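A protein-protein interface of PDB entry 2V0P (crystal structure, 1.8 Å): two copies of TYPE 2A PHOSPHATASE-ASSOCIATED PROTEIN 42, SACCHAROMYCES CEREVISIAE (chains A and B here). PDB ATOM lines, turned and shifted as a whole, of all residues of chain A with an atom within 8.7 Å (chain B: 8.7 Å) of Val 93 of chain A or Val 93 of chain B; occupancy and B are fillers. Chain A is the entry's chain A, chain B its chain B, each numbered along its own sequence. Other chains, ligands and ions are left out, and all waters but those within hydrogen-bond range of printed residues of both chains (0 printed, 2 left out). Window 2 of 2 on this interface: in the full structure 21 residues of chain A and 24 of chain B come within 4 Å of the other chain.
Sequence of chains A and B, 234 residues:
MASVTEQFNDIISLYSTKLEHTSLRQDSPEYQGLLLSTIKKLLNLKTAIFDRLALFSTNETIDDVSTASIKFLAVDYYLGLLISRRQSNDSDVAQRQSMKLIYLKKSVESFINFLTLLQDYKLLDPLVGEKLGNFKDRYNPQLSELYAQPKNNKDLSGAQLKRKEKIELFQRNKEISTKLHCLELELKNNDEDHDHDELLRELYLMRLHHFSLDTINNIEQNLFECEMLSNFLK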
ATOM      1  N   SER A  88     -16.348  19.626 -11.657  1.00  0.00           N
ATOM      2  CA  SER A  88     -17.816  19.726 -11.728  1.00  0.00           C
ATOM      3  C   SER A  88     -18.274  20.985 -11.016  1.00  0.00           C
ATOM      4  O   SER A  88     -17.590  21.464 -10.114  1.00  0.00           O
ATOM      5  CB  SER A  88     -18.450  18.501 -11.115  1.00  0.00           C
ATOM      6  OG  SER A  88     -19.812  18.720 -10.871  1.00  0.00           O
ATOM      7  N   ASN A  89     -19.412  21.519 -11.437  1.00  0.00           N
ATOM      8  CA  ASN A  89     -20.069  22.637 -10.744  1.00  0.00           C
ATOM      9  C   ASN A  89     -21.447  22.261 -10.171  1.00  0.00           C
ATOM     10  O   ASN A  89     -22.198  23.119  -9.678  1.00  0.00           O
ATOM     11  CB  ASN A  89     -20.148  23.871 -11.657  1.00  0.00           C
ATOM     12  CG  ASN A  89     -18.830  24.652 -11.693  1.00  0.00           C
ATOM     13  OD1 ASN A  89     -18.275  24.920 -12.769  1.00  0.00           O
ATOM     14  ND2 ASN A  89     -18.318  25.012 -10.503  1.00  0.00           N
ATOM     15  N   ASP A  90     -21.766  20.973 -10.233  1.00  0.00           N
ATOM     16  CA  ASP A  90     -22.970  20.448  -9.635  1.00  0.00           C
ATOM     17  C   ASP A  90     -23.206  21.056  -8.238  1.00  0.00           C
ATOM     18  O   ASP A  90     -22.283  21.182  -7.443  1.00  0.00           O
ATOM     19  CB  ASP A  90     -22.902  18.924  -9.559  1.00  0.00           C
ATOM     20  CG  ASP A  90     -24.279  18.282  -9.368  1.00  0.00           C
ATOM     21  OD1 ASP A  90     -24.829  17.745 -10.354  1.00  0.00           O
ATOM     22  OD2 ASP A  90     -24.821  18.326  -8.242  1.00  0.00           O
ATOM     23  N   SER A  91     -24.442  21.455  -7.960  1.00  0.00           N
ATOM     24  CA  SER A  91     -24.770  22.028  -6.644  1.00  0.00           C
ATOM     25  C   SER A  91     -24.583  21.001  -5.530  1.00  0.00           C
ATOM     26  O   SER A  91     -24.253  21.350  -4.393  1.00  0.00           O
ATOM     27  CB  SER A  91     -26.181  22.610  -6.626  1.00  0.00           C
ATOM     28  OG  SER A  91     -27.098  21.752  -7.277  1.00  0.00           O
ATOM     29  N   ASP A  92     -24.779  19.731  -5.875  1.00  0.00           N
ATOM     30  CA  ASP A  92     -24.581  18.627  -4.937  1.00  0.00           C
ATOM     31  C   ASP A  92     -23.091  18.457  -4.642  1.00  0.00           C
ATOM     32  O   ASP A  92     -22.264  18.131  -5.540  1.00  0.00           O
ATOM     33  CB  ASP A  92     -25.197  17.341  -5.503  1.00  0.00           C
ATOM     34  CG  ASP A  92     -25.324  16.245  -4.472  1.00  0.00           C
ATOM     35  OD1 ASP A  92     -24.391  16.062  -3.676  1.00  0.00           O
ATOM     36  OD2 ASP A  92     -26.364  15.551  -4.468  1.00  0.00           O
ATOM     37  N   VAL A  93     -22.741  18.712  -3.392  1.00  0.00           N
ATOM     38  CA  VAL A  93     -21.338  18.646  -2.964  1.00  0.00           C
ATOM     39  C   VAL A  93     -20.706  17.256  -3.089  1.00  0.00           C
ATOM     40  O   VAL A  93     -19.594  17.164  -3.496  1.00  0.00           O
ATOM     41  CB  VAL A  93     -21.122  19.212  -1.517  1.00  0.00           C
ATOM     42  CG1 VAL A  93     -19.987  18.501  -0.806  1.00  0.00           C
ATOM     43  CG2 VAL A  93     -20.844  20.704  -1.567  1.00  0.00           C
ATOM     44  N   ALA A  94     -21.425  16.194  -2.741  1.00  0.00           N
ATOM     45  CA  ALA A  94     -20.921  14.829  -2.907  1.00  0.00           C
ATOM     46  C   ALA A  94     -20.628  14.523  -4.381  1.00  0.00           C
ATOM     47  O   ALA A  94     -19.593  13.918  -4.712  1.00  0.00           O
ATOM     48  CB  ALA A  94     -21.915  13.811  -2.319  1.00  0.00           C
ATOM     49  N   GLN A  95     -21.519  14.995  -5.248  1.00  0.00           N
ATOM     50  CA  GLN A  95     -21.488  14.692  -6.656  1.00  0.00           C
ATOM     51  C   GLN A  95     -20.315  15.370  -7.328  1.00  0.00           C
ATOM     52  O   GLN A  95     -19.638  14.780  -8.169  1.00  0.00           O
ATOM     53  CB  GLN A  95     -22.796  15.123  -7.322  1.00  0.00           C
ATOM     54  CG  GLN A  95     -23.981  14.296  -6.911  1.00  0.00           C
ATOM     55  CD  GLN A  95     -23.946  12.886  -7.468  1.00  0.00           C
ATOM     56  OE1 GLN A  95     -24.030  11.911  -6.715  1.00  0.00           O
ATOM     57  NE2 GLN A  95     -23.850  12.771  -8.793  1.00  0.00           N
ATOM     58  N   ARG A  96     -20.084  16.608  -6.929  1.00  0.00           N
ATOM     59  CA  ARG A  96     -19.007  17.408  -7.434  1.00  0.00           C
ATOM     60  C   ARG A  96     -17.626  16.901  -7.001  1.00  0.00           C
ATOM     61  O   ARG A  96     -16.746  16.777  -7.860  1.00  0.00           O
ATOM     62  CB  ARG A  96     -19.326  18.900  -7.262  1.00  0.00           C
ATOM     63  CG  ARG A  96     -18.430  19.802  -6.522  1.00  0.00           C
ATOM     64  CD  ARG A  96     -19.084  21.165  -6.533  1.00  0.00           C
ATOM     65  NE  ARG A  96     -19.104  21.830  -5.228  1.00  0.00           N
ATOM     66  CZ  ARG A  96     -20.087  22.622  -4.819  1.00  0.00           C
ATOM     67  NH1 ARG A  96     -21.140  22.846  -5.604  1.00  0.00           N
ATOM     68  NH2 ARG A  96     -20.030  23.190  -3.617  1.00  0.00           N
ATOM     69  N   GLN A  97     -17.494  16.486  -5.736  1.00  0.00           N
ATOM     70  CA  GLN A  97     -16.323  15.870  -5.262  1.00  0.00           C
ATOM     71  C   GLN A  97     -16.089  14.488  -5.837  1.00  0.00           C
ATOM     72  O   GLN A  97     -14.941  14.148  -6.177  1.00  0.00           O
ATOM     73  CB  GLN A  97     -16.237  15.876  -3.724  1.00  0.00           C
ATOM     74  CG  GLN A  97     -16.032  17.281  -3.163  1.00  0.00           C
ATOM     75  CD  GLN A  97     -16.104  17.333  -1.670  1.00  0.00           C
ATOM     76  OE1 GLN A  97     -15.749  16.373  -0.996  1.00  0.00           O
ATOM     77  NE2 GLN A  97     -16.613  18.447  -1.135  1.00  0.00           N
ATOM     78  N   SER A  98     -17.147  13.702  -5.956  1.00  0.00           N
ATOM     79  CA  SER A  98     -17.020  12.373  -6.535  1.00  0.00           C
ATOM     80  C   SER A  98     -16.558  12.450  -8.007  1.00  0.00           C
ATOM     81  O   SER A  98     -15.696  11.718  -8.409  1.00  0.00           O
ATOM     82  CB  SER A  98     -18.330  11.613  -6.445  1.00  0.00           C
ATOM     83  OG  SER A  98     -18.696  11.358  -5.081  1.00  0.00           O
ATOM     84  N   MET A  99     -17.166  13.341  -8.771  1.00  0.00           N
ATOM     85  CA  MET A  99     -16.767  13.636 -10.168  1.00  0.00           C
ATOM     86  C   MET A  99     -15.256  13.932 -10.271  1.00  0.00           C
ATOM     87  O   MET A  99     -14.581  13.425 -11.141  1.00  0.00           O
ATOM     88  CB  MET A  99     -17.577  14.801 -10.725  1.00  0.00           C
ATOM     89  CG  MET A  99     -18.797  14.427 -11.535  1.00  0.00           C
ATOM     90  SD  MET A  99     -18.474  13.065 -12.928  1.00  0.00           S
ATOM     91  CE  MET A  99     -16.846  13.520 -13.735  1.00  0.00           C
ATOM     92  N   LYS A 100     -14.714  14.729  -9.361  1.00  0.00           N
ATOM     93  CA  LYS A 100     -13.278  14.991  -9.374  1.00  0.00           C
ATOM     94  C   LYS A 100     -12.448  13.717  -9.374  1.00  0.00           C
ATOM     95  O   LYS A 100     -11.477  13.644 -10.084  1.00  0.00           O
ATOM     96  CB  LYS A 100     -12.831  15.960  -8.258  1.00  0.00           C
ATOM     97  CG  LYS A 100     -11.363  16.397  -8.420  1.00  0.00           C
ATOM     98  CD  LYS A 100     -11.197  17.448  -9.503  1.00  0.00           C
ATOM     99  CE  LYS A 100      -9.723  17.743  -9.710  1.00  0.00           C
ATOM    100  NZ  LYS A 100      -9.492  18.244 -11.105  1.00  0.00           N
ATOM    101  N   PHE A 232     -11.763  12.560   2.284  1.00  0.00           N
ATOM    102  CA  PHE A 232     -12.748  13.537   2.697  1.00  0.00           C
ATOM    103  C   PHE A 232     -14.195  13.215   2.279  1.00  0.00           C
ATOM    104  O   PHE A 232     -15.134  13.873   2.733  1.00  0.00           O
ATOM    105  CB  PHE A 232     -12.299  14.918   2.242  1.00  0.00           C
ATOM    106  CG  PHE A 232     -11.085  15.396   2.959  1.00  0.00           C
ATOM    107  CD1 PHE A 232     -11.140  15.674   4.322  1.00  0.00           C
ATOM    108  CD2 PHE A 232      -9.878  15.525   2.303  1.00  0.00           C
ATOM    109  CE1 PHE A 232     -10.015  16.101   5.002  1.00  0.00           C
ATOM    110  CE2 PHE A 232      -8.757  15.951   2.977  1.00  0.00           C
ATOM    111  CZ  PHE A 232      -8.828  16.245   4.316  1.00  0.00           C
ATOM    112  N   LEU A 233     -14.363  12.203   1.431  1.00  0.00           N
ATOM    113  CA  LEU A 233     -15.693  11.708   1.061  1.00  0.00           C
ATOM    114  C   LEU A 233     -16.073  10.450   1.848  1.00  0.00           C
ATOM    115  O   LEU A 233     -17.262  10.157   2.042  1.00  0.00           O
ATOM    116  CB  LEU A 233     -15.782  11.459  -0.451  1.00  0.00           C
ATOM    117  CG  LEU A 233     -15.981  12.685  -1.350  1.00  0.00           C
ATOM    118  CD1 LEU A 233     -15.777  12.302  -2.834  1.00  0.00           C
ATOM    119  CD2 LEU A 233     -17.347  13.391  -1.132  1.00  0.00           C
ATOM    120  N   LYS A 234     -15.056   9.726   2.314  1.00  0.00           N
ATOM    121  CA  LYS A 234     -15.250   8.539   3.155  1.00  0.00           C
ATOM    122  C   LYS A 234     -15.884   8.884   4.507  1.00  0.00           C
ATOM    123  O   LYS A 234     -16.176   8.001   5.322  1.00  0.00           O
ATOM    124  CB  LYS A 234     -13.918   7.804   3.372  1.00  0.00           C
ATOM    125  CG  LYS A 234     -13.333   7.146   2.115  1.00  0.00           C
ATOM    126  CD  LYS A 234     -12.393   5.993   2.471  1.00  0.00           C
ATOM    127  CE  LYS A 234     -13.164   4.799   3.054  1.00  0.00           C
ATOM    128  NZ  LYS A 234     -12.332   3.968   3.978  1.00  0.00           N
ATOM    129  OXT LYS A 234     -16.122  10.052   4.835  1.00  0.00           O
ATOM    130  N   SER B  88     -18.016  13.430  12.265  1.00  0.00           N
ATOM    131  CA  SER B  88     -19.464  13.423  12.138  1.00  0.00           C
ATOM    132  C   SER B  88     -19.919  12.207  11.317  1.00  0.00           C
ATOM    133  O   SER B  88     -19.215  11.774  10.390  1.00  0.00           O
ATOM    134  CB  SER B  88     -19.916  14.717  11.470  1.00  0.00           C
ATOM    135  OG  SER B  88     -21.301  14.712  11.277  1.00  0.00           O
ATOM    136  N   ASN B  89     -21.087  11.655  11.656  1.00  0.00           N
ATOM    137  CA  ASN B  89     -21.676  10.583  10.853  1.00  0.00           C
ATOM    138  C   ASN B  89     -23.007  10.989  10.217  1.00  0.00           C
ATOM    139  O   ASN B  89     -23.784  10.149   9.769  1.00  0.00           O
ATOM    140  CB  ASN B  89     -21.797   9.273  11.650  1.00  0.00           C
ATOM    141  CG  ASN B  89     -22.470   9.464  12.990  1.00  0.00           C
ATOM    142  OD1 ASN B  89     -23.681   9.701  13.063  1.00  0.00           O
ATOM    143  ND2 ASN B  89     -21.689   9.343  14.070  1.00  0.00           N
ATOM    144  N   ASP B  90     -23.240  12.298  10.177  1.00  0.00           N
ATOM    145  CA  ASP B  90     -24.368  12.879   9.474  1.00  0.00           C
ATOM    146  C   ASP B  90     -24.394  12.426   8.013  1.00  0.00           C
ATOM    147  O   ASP B  90     -23.343  12.230   7.388  1.00  0.00           O
ATOM    148  CB  ASP B  90     -24.298  14.399   9.533  1.00  0.00           C
ATOM    149  CG  ASP B  90     -25.632  15.046   9.224  1.00  0.00           C
ATOM    150  OD1 ASP B  90     -25.845  15.455   8.062  1.00  0.00           O
ATOM    151  OD2 ASP B  90     -26.482  15.102  10.131  1.00  0.00           O
ATOM    152  N   SER B  91     -25.596  12.269   7.473  1.00  0.00           N
ATOM    153  CA  SER B  91     -25.765  11.823   6.095  1.00  0.00           C
ATOM    154  C   SER B  91     -25.287  12.875   5.102  1.00  0.00           C
ATOM    155  O   SER B  91     -24.904  12.542   3.983  1.00  0.00           O
ATOM    156  CB  SER B  91     -27.238  11.492   5.826  1.00  0.00           C
ATOM    157  OG  SER B  91     -27.758  10.631   6.832  1.00  0.00           O
ATOM    158  N   ASP B  92     -25.336  14.143   5.503  1.00  0.00           N
ATOM    159  CA  ASP B  92     -24.938  15.246   4.638  1.00  0.00           C
ATOM    160  C   ASP B  92     -23.406  15.449   4.601  1.00  0.00           C
ATOM    161  O   ASP B  92     -22.770  15.782   5.602  1.00  0.00           O
ATOM    162  CB  ASP B  92     -25.657  16.533   5.041  1.00  0.00           C
ATOM    163  CG  ASP B  92     -25.456  17.650   4.052  1.00  0.00           C
ATOM    164  OD1 ASP B  92     -25.753  17.466   2.844  1.00  0.00           O
ATOM    165  OD2 ASP B  92     -25.019  18.733   4.479  1.00  0.00           O
ATOM    166  N   VAL B  93     -22.837  15.251   3.423  1.00  0.00           N
ATOM    167  CA  VAL B  93     -21.413  15.374   3.207  1.00  0.00           C
ATOM    168  C   VAL B  93     -20.871  16.729   3.595  1.00  0.00           C
ATOM    169  O   VAL B  93     -19.833  16.786   4.271  1.00  0.00           O
ATOM    170  CB  VAL B  93     -21.048  15.002   1.734  1.00  0.00           C
ATOM    171  CG1 VAL B  93     -19.933  15.880   1.187  1.00  0.00           C
ATOM    172  CG2 VAL B  93     -20.646  13.557   1.673  1.00  0.00           C
ATOM    173  N   ALA B  94     -21.545  17.816   3.203  1.00  0.00           N
ATOM    174  CA  ALA B  94     -21.055  19.151   3.596  1.00  0.00           C
ATOM    175  C   ALA B  94     -20.987  19.346   5.130  1.00  0.00           C
ATOM    176  O   ALA B  94     -20.052  19.973   5.632  1.00  0.00           O
ATOM    177  CB  ALA B  94     -21.834  20.232   2.982  1.00  0.00           C
ATOM    178  N   GLN B  95     -21.974  18.831   5.846  1.00  0.00           N
ATOM    179  CA  GLN B  95     -21.969  18.929   7.325  1.00  0.00           C
ATOM    180  C   GLN B  95     -20.767  18.194   7.950  1.00  0.00           C
ATOM    181  O   GLN B  95     -20.039  18.774   8.740  1.00  0.00           O
ATOM    182  CB  GLN B  95     -23.303  18.463   7.915  1.00  0.00           C
ATOM    183  CG  GLN B  95     -23.438  18.853   9.393  1.00  0.00           C
ATOM    184  CD  GLN B  95     -24.812  18.579   9.986  1.00  0.00           C
ATOM    185  OE1 GLN B  95     -25.840  18.989   9.434  1.00  0.00           O
ATOM    186  NE2 GLN B  95     -24.830  17.915  11.150  1.00  0.00           N
ATOM    187  N   ARG B  96     -20.564  16.942   7.563  1.00  0.00           N
ATOM    188  CA  ARG B  96     -19.441  16.116   7.968  1.00  0.00           C
ATOM    189  C   ARG B  96     -18.127  16.831   7.739  1.00  0.00           C
ATOM    190  O   ARG B  96     -17.363  17.014   8.669  1.00  0.00           O
ATOM    191  CB  ARG B  96     -19.379  14.796   7.219  1.00  0.00           C
ATOM    192  CG  ARG B  96     -20.530  13.831   7.446  1.00  0.00           C
ATOM    193  CD  ARG B  96     -20.110  12.376   7.173  1.00  0.00           C
ATOM    194  NE  ARG B  96     -19.740  12.102   5.780  1.00  0.00           N
ATOM    195  CZ  ARG B  96     -20.595  11.797   4.806  1.00  0.00           C
ATOM    196  NH1 ARG B  96     -21.903  11.744   5.038  1.00  0.00           N
ATOM    197  NH2 ARG B  96     -20.138  11.549   3.585  1.00  0.00           N
ATOM    198  N   GLN B  97     -17.916  17.286   6.508  1.00  0.00           N
ATOM    199  CA  GLN B  97     -16.698  17.975   6.153  1.00  0.00           C
ATOM    200  C   GLN B  97     -16.516  19.261   6.981  1.00  0.00           C
ATOM    201  O   GLN B  97     -15.407  19.555   7.431  1.00  0.00           O
ATOM    202  CB  GLN B  97     -16.670  18.205   4.615  1.00  0.00           C
ATOM    203  CG  GLN B  97     -16.346  16.924   3.838  1.00  0.00           C
ATOM    204  CD  GLN B  97     -16.310  17.122   2.305  1.00  0.00           C
ATOM    205  OE1 GLN B  97     -16.320  18.234   1.833  1.00  0.00           O
ATOM    206  NE2 GLN B  97     -16.249  16.042   1.555  1.00  0.00           N
ATOM    207  N   SER B  98     -17.595  20.021   7.203  1.00  0.00           N
ATOM    208  CA  SER B  98     -17.427  21.240   7.964  1.00  0.00           C
ATOM    209  C   SER B  98     -17.169  20.882   9.453  1.00  0.00           C
ATOM    210  O   SER B  98     -16.324  21.499  10.096  1.00  0.00           O
ATOM    211  CB  SER B  98     -18.615  22.189   7.794  1.00  0.00           C
ATOM    212  OG  SER B  98     -18.746  22.567   6.441  1.00  0.00           O
ATOM    213  N   MET B  99     -17.809  19.820   9.923  1.00  0.00           N
ATOM    214  CA  MET B  99     -17.612  19.371  11.279  1.00  0.00           C
ATOM    215  C   MET B  99     -16.196  18.908  11.418  1.00  0.00           C
ATOM    216  O   MET B  99     -15.571  19.349  12.297  1.00  0.00           O
ATOM    217  CB  MET B  99     -18.627  18.318  11.709  1.00  0.00           C
ATOM    218  CG  MET B  99     -19.979  18.927  11.933  1.00  0.00           C
ATOM    219  SD  MET B  99     -20.092  19.840  13.660  1.00  0.00           S
ATOM    220  CE  MET B  99     -20.009  18.220  14.745  1.00  0.00           C
ATOM    221  N   LYS B 100     -15.686  18.102  10.471  1.00  0.00           N
ATOM    222  CA  LYS B 100     -14.248  17.759  10.430  1.00  0.00           C
ATOM    223  C   LYS B 100     -13.323  18.989  10.441  1.00  0.00           C
ATOM    224  O   LYS B 100     -12.431  19.031  11.231  1.00  0.00           O
ATOM    225  CB  LYS B 100     -13.904  16.865   9.228  1.00  0.00           C
ATOM    226  CG  LYS B 100     -12.439  16.443   9.158  1.00  0.00           C
ATOM    227  CD  LYS B 100     -12.166  15.288  10.111  1.00  0.00           C
ATOM    228  CE  LYS B 100     -10.710  15.125  10.472  1.00  0.00           C
ATOM    229  NZ  LYS B 100     -10.588  14.001  11.457  1.00  0.00           N
ATOM    230  N   LEU B 229     -10.150  21.098   3.093  1.00  0.00           N
ATOM    231  CA  LEU B 229     -11.541  21.265   3.437  1.00  0.00           C
ATOM    232  C   LEU B 229     -12.010  22.690   3.134  1.00  0.00           C
ATOM    233  O   LEU B 229     -13.058  22.882   2.515  1.00  0.00           O
ATOM    234  CB  LEU B 229     -11.745  20.910   4.911  1.00  0.00           C
ATOM    235  CG  LEU B 229     -11.679  19.424   5.278  1.00  0.00           C
ATOM    236  CD1 LEU B 229     -11.511  19.280   6.779  1.00  0.00           C
ATOM    237  CD2 LEU B 229     -12.919  18.656   4.798  1.00  0.00           C
ATOM    238  N   PHE B 232     -12.810  23.525  -0.570  1.00  0.00           N
ATOM    239  CA  PHE B 232     -14.166  23.075  -0.908  1.00  0.00           C
ATOM    240  C   PHE B 232     -15.257  24.145  -0.778  1.00  0.00           C
ATOM    241  O   PHE B 232     -16.301  24.036  -1.424  1.00  0.00           O
ATOM    242  CB  PHE B 232     -14.565  21.855  -0.073  1.00  0.00           C
ATOM    243  CG  PHE B 232     -13.804  20.611  -0.398  1.00  0.00           C
ATOM    244  CD1 PHE B 232     -13.471  19.713   0.612  1.00  0.00           C
ATOM    245  CD2 PHE B 232     -13.413  20.325  -1.709  1.00  0.00           C
ATOM    246  CE1 PHE B 232     -12.769  18.551   0.328  1.00  0.00           C
ATOM    247  CE2 PHE B 232     -12.705  19.171  -1.997  1.00  0.00           C
ATOM    248  CZ  PHE B 232     -12.381  18.280  -0.980  1.00  0.00           C
ATOM    249  N   LEU B 233     -15.019  25.152   0.070  1.00  0.00           N
ATOM    250  CA  LEU B 233     -15.931  26.295   0.262  1.00  0.00           C
ATOM    251  C   LEU B 233     -15.500  27.533  -0.543  1.00  0.00           C
ATOM    252  O   LEU B 233     -16.349  28.268  -1.059  1.00  0.00           O
ATOM    253  CB  LEU B 233     -16.051  26.669   1.752  1.00  0.00           C
ATOM    254  CG  LEU B 233     -16.497  25.621   2.785  1.00  0.00           C
ATOM    255  CD1 LEU B 233     -16.133  26.060   4.209  1.00  0.00           C
ATOM    256  CD2 LEU B 233     -17.992  25.298   2.667  1.00  0.00           C
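NH1 of Arg 96 of chain B lies within hydrogen-bond range of O of Ser 91 of chain B, 3.3 Å away.
The guanidinium group (NH1) of Arg 96 of chain B lies within hydrogen-bond range of the backbone carbonyl oxygen (O) of Asp 90 of chain B (2.8 Å).
Hydrophobic or aromatic side chains of chain A within 4 Å of the printed part of chain B: Val 93, Phe 232 and Leu 233.
Among the printed residues, 7 pairs touch across the chains.
Of chain B, only Val 93 comes within 4 Å of Val 93 of chain A.
Ala 94 of chain A touches none of the printed residues of chain B.
Printed residues of chain B within 4 Å of Gln 97 of chain A: Gln 97 (2.6 Å) and Phe 232 (3.6 Å).
Printed residues of chain B within 4 Å of Leu 233 of chain A: Arg 96 and Gln 97.
No residue of chain A comes within 4 Å of Asp 92 of chain B.
Of chain A, only Val 93 comes within 4 Å of Val 93 of chain B.
Of the printed residues of chain A, Gln 97 of chain B touches Gln 97 (2.6 Å), Phe 232 (2.7 Å) and Leu 233 (3.9 Å).
Printed residues of chain A within 4 Å of Leu 229 of chain B: Phe 232 (3.5 Å).
Printed residues of chain A within 4 Å of Phe 232 of chain B: Gln 97.
Leu 233 of chain B touches none of the printed residues of chain A.
The nearest residue of chain A that does not touch Val 93 of chain B is Ala 94 of chain A (4.2 Å).
The nearest printed residue of chain A that does not touch Phe 232 of chain B is Phe 232 of chain A (4.1 Å).
The side-chain amide nitrogen (NE2) of Gln 97 of chain B sits at hydrogen-bond distance from the backbone carbonyl oxygen (O) of Phe 232 of chain A (2.7 Å).
NE2 of Gln 97 of chain B lies within hydrogen-bond range of OE1 of Gln 97 of chain A (2.6 Å).
Among the printed residues, merely in contact across the chains: Val 93 of chain A with Val 93 of chain B (3.3 Å), Gln 97 of chain A with Phe 232 of chain B (3.6 Å), Phe 232 of chain A with Leu 229 of chain B (3.5 Å), Leu 233 of chain A with Arg 96 of chain B (3.5 Å) and Leu 233 of chain A with Gln 97 of chain B (3.9 Å).
Val 93 of chain A touches its own counterpart, Val 93 of chain B.
Gln 97 of chain A touches Phe 232 of chain B, and with the chains exchanged Phe 232 of chain A touches Gln 97 of chain B.
Leu 233 of chain A touches Arg 96 of chain B, but with the chains exchanged Arg 96 of chain A does not touch Leu 233 of chain B (6.4 Å).
Leu 233 of chain A touches Gln 97 of chain B, but with the chains exchanged Gln 97 of chain A does not touch Leu 233 of chain B (7.0 Å).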
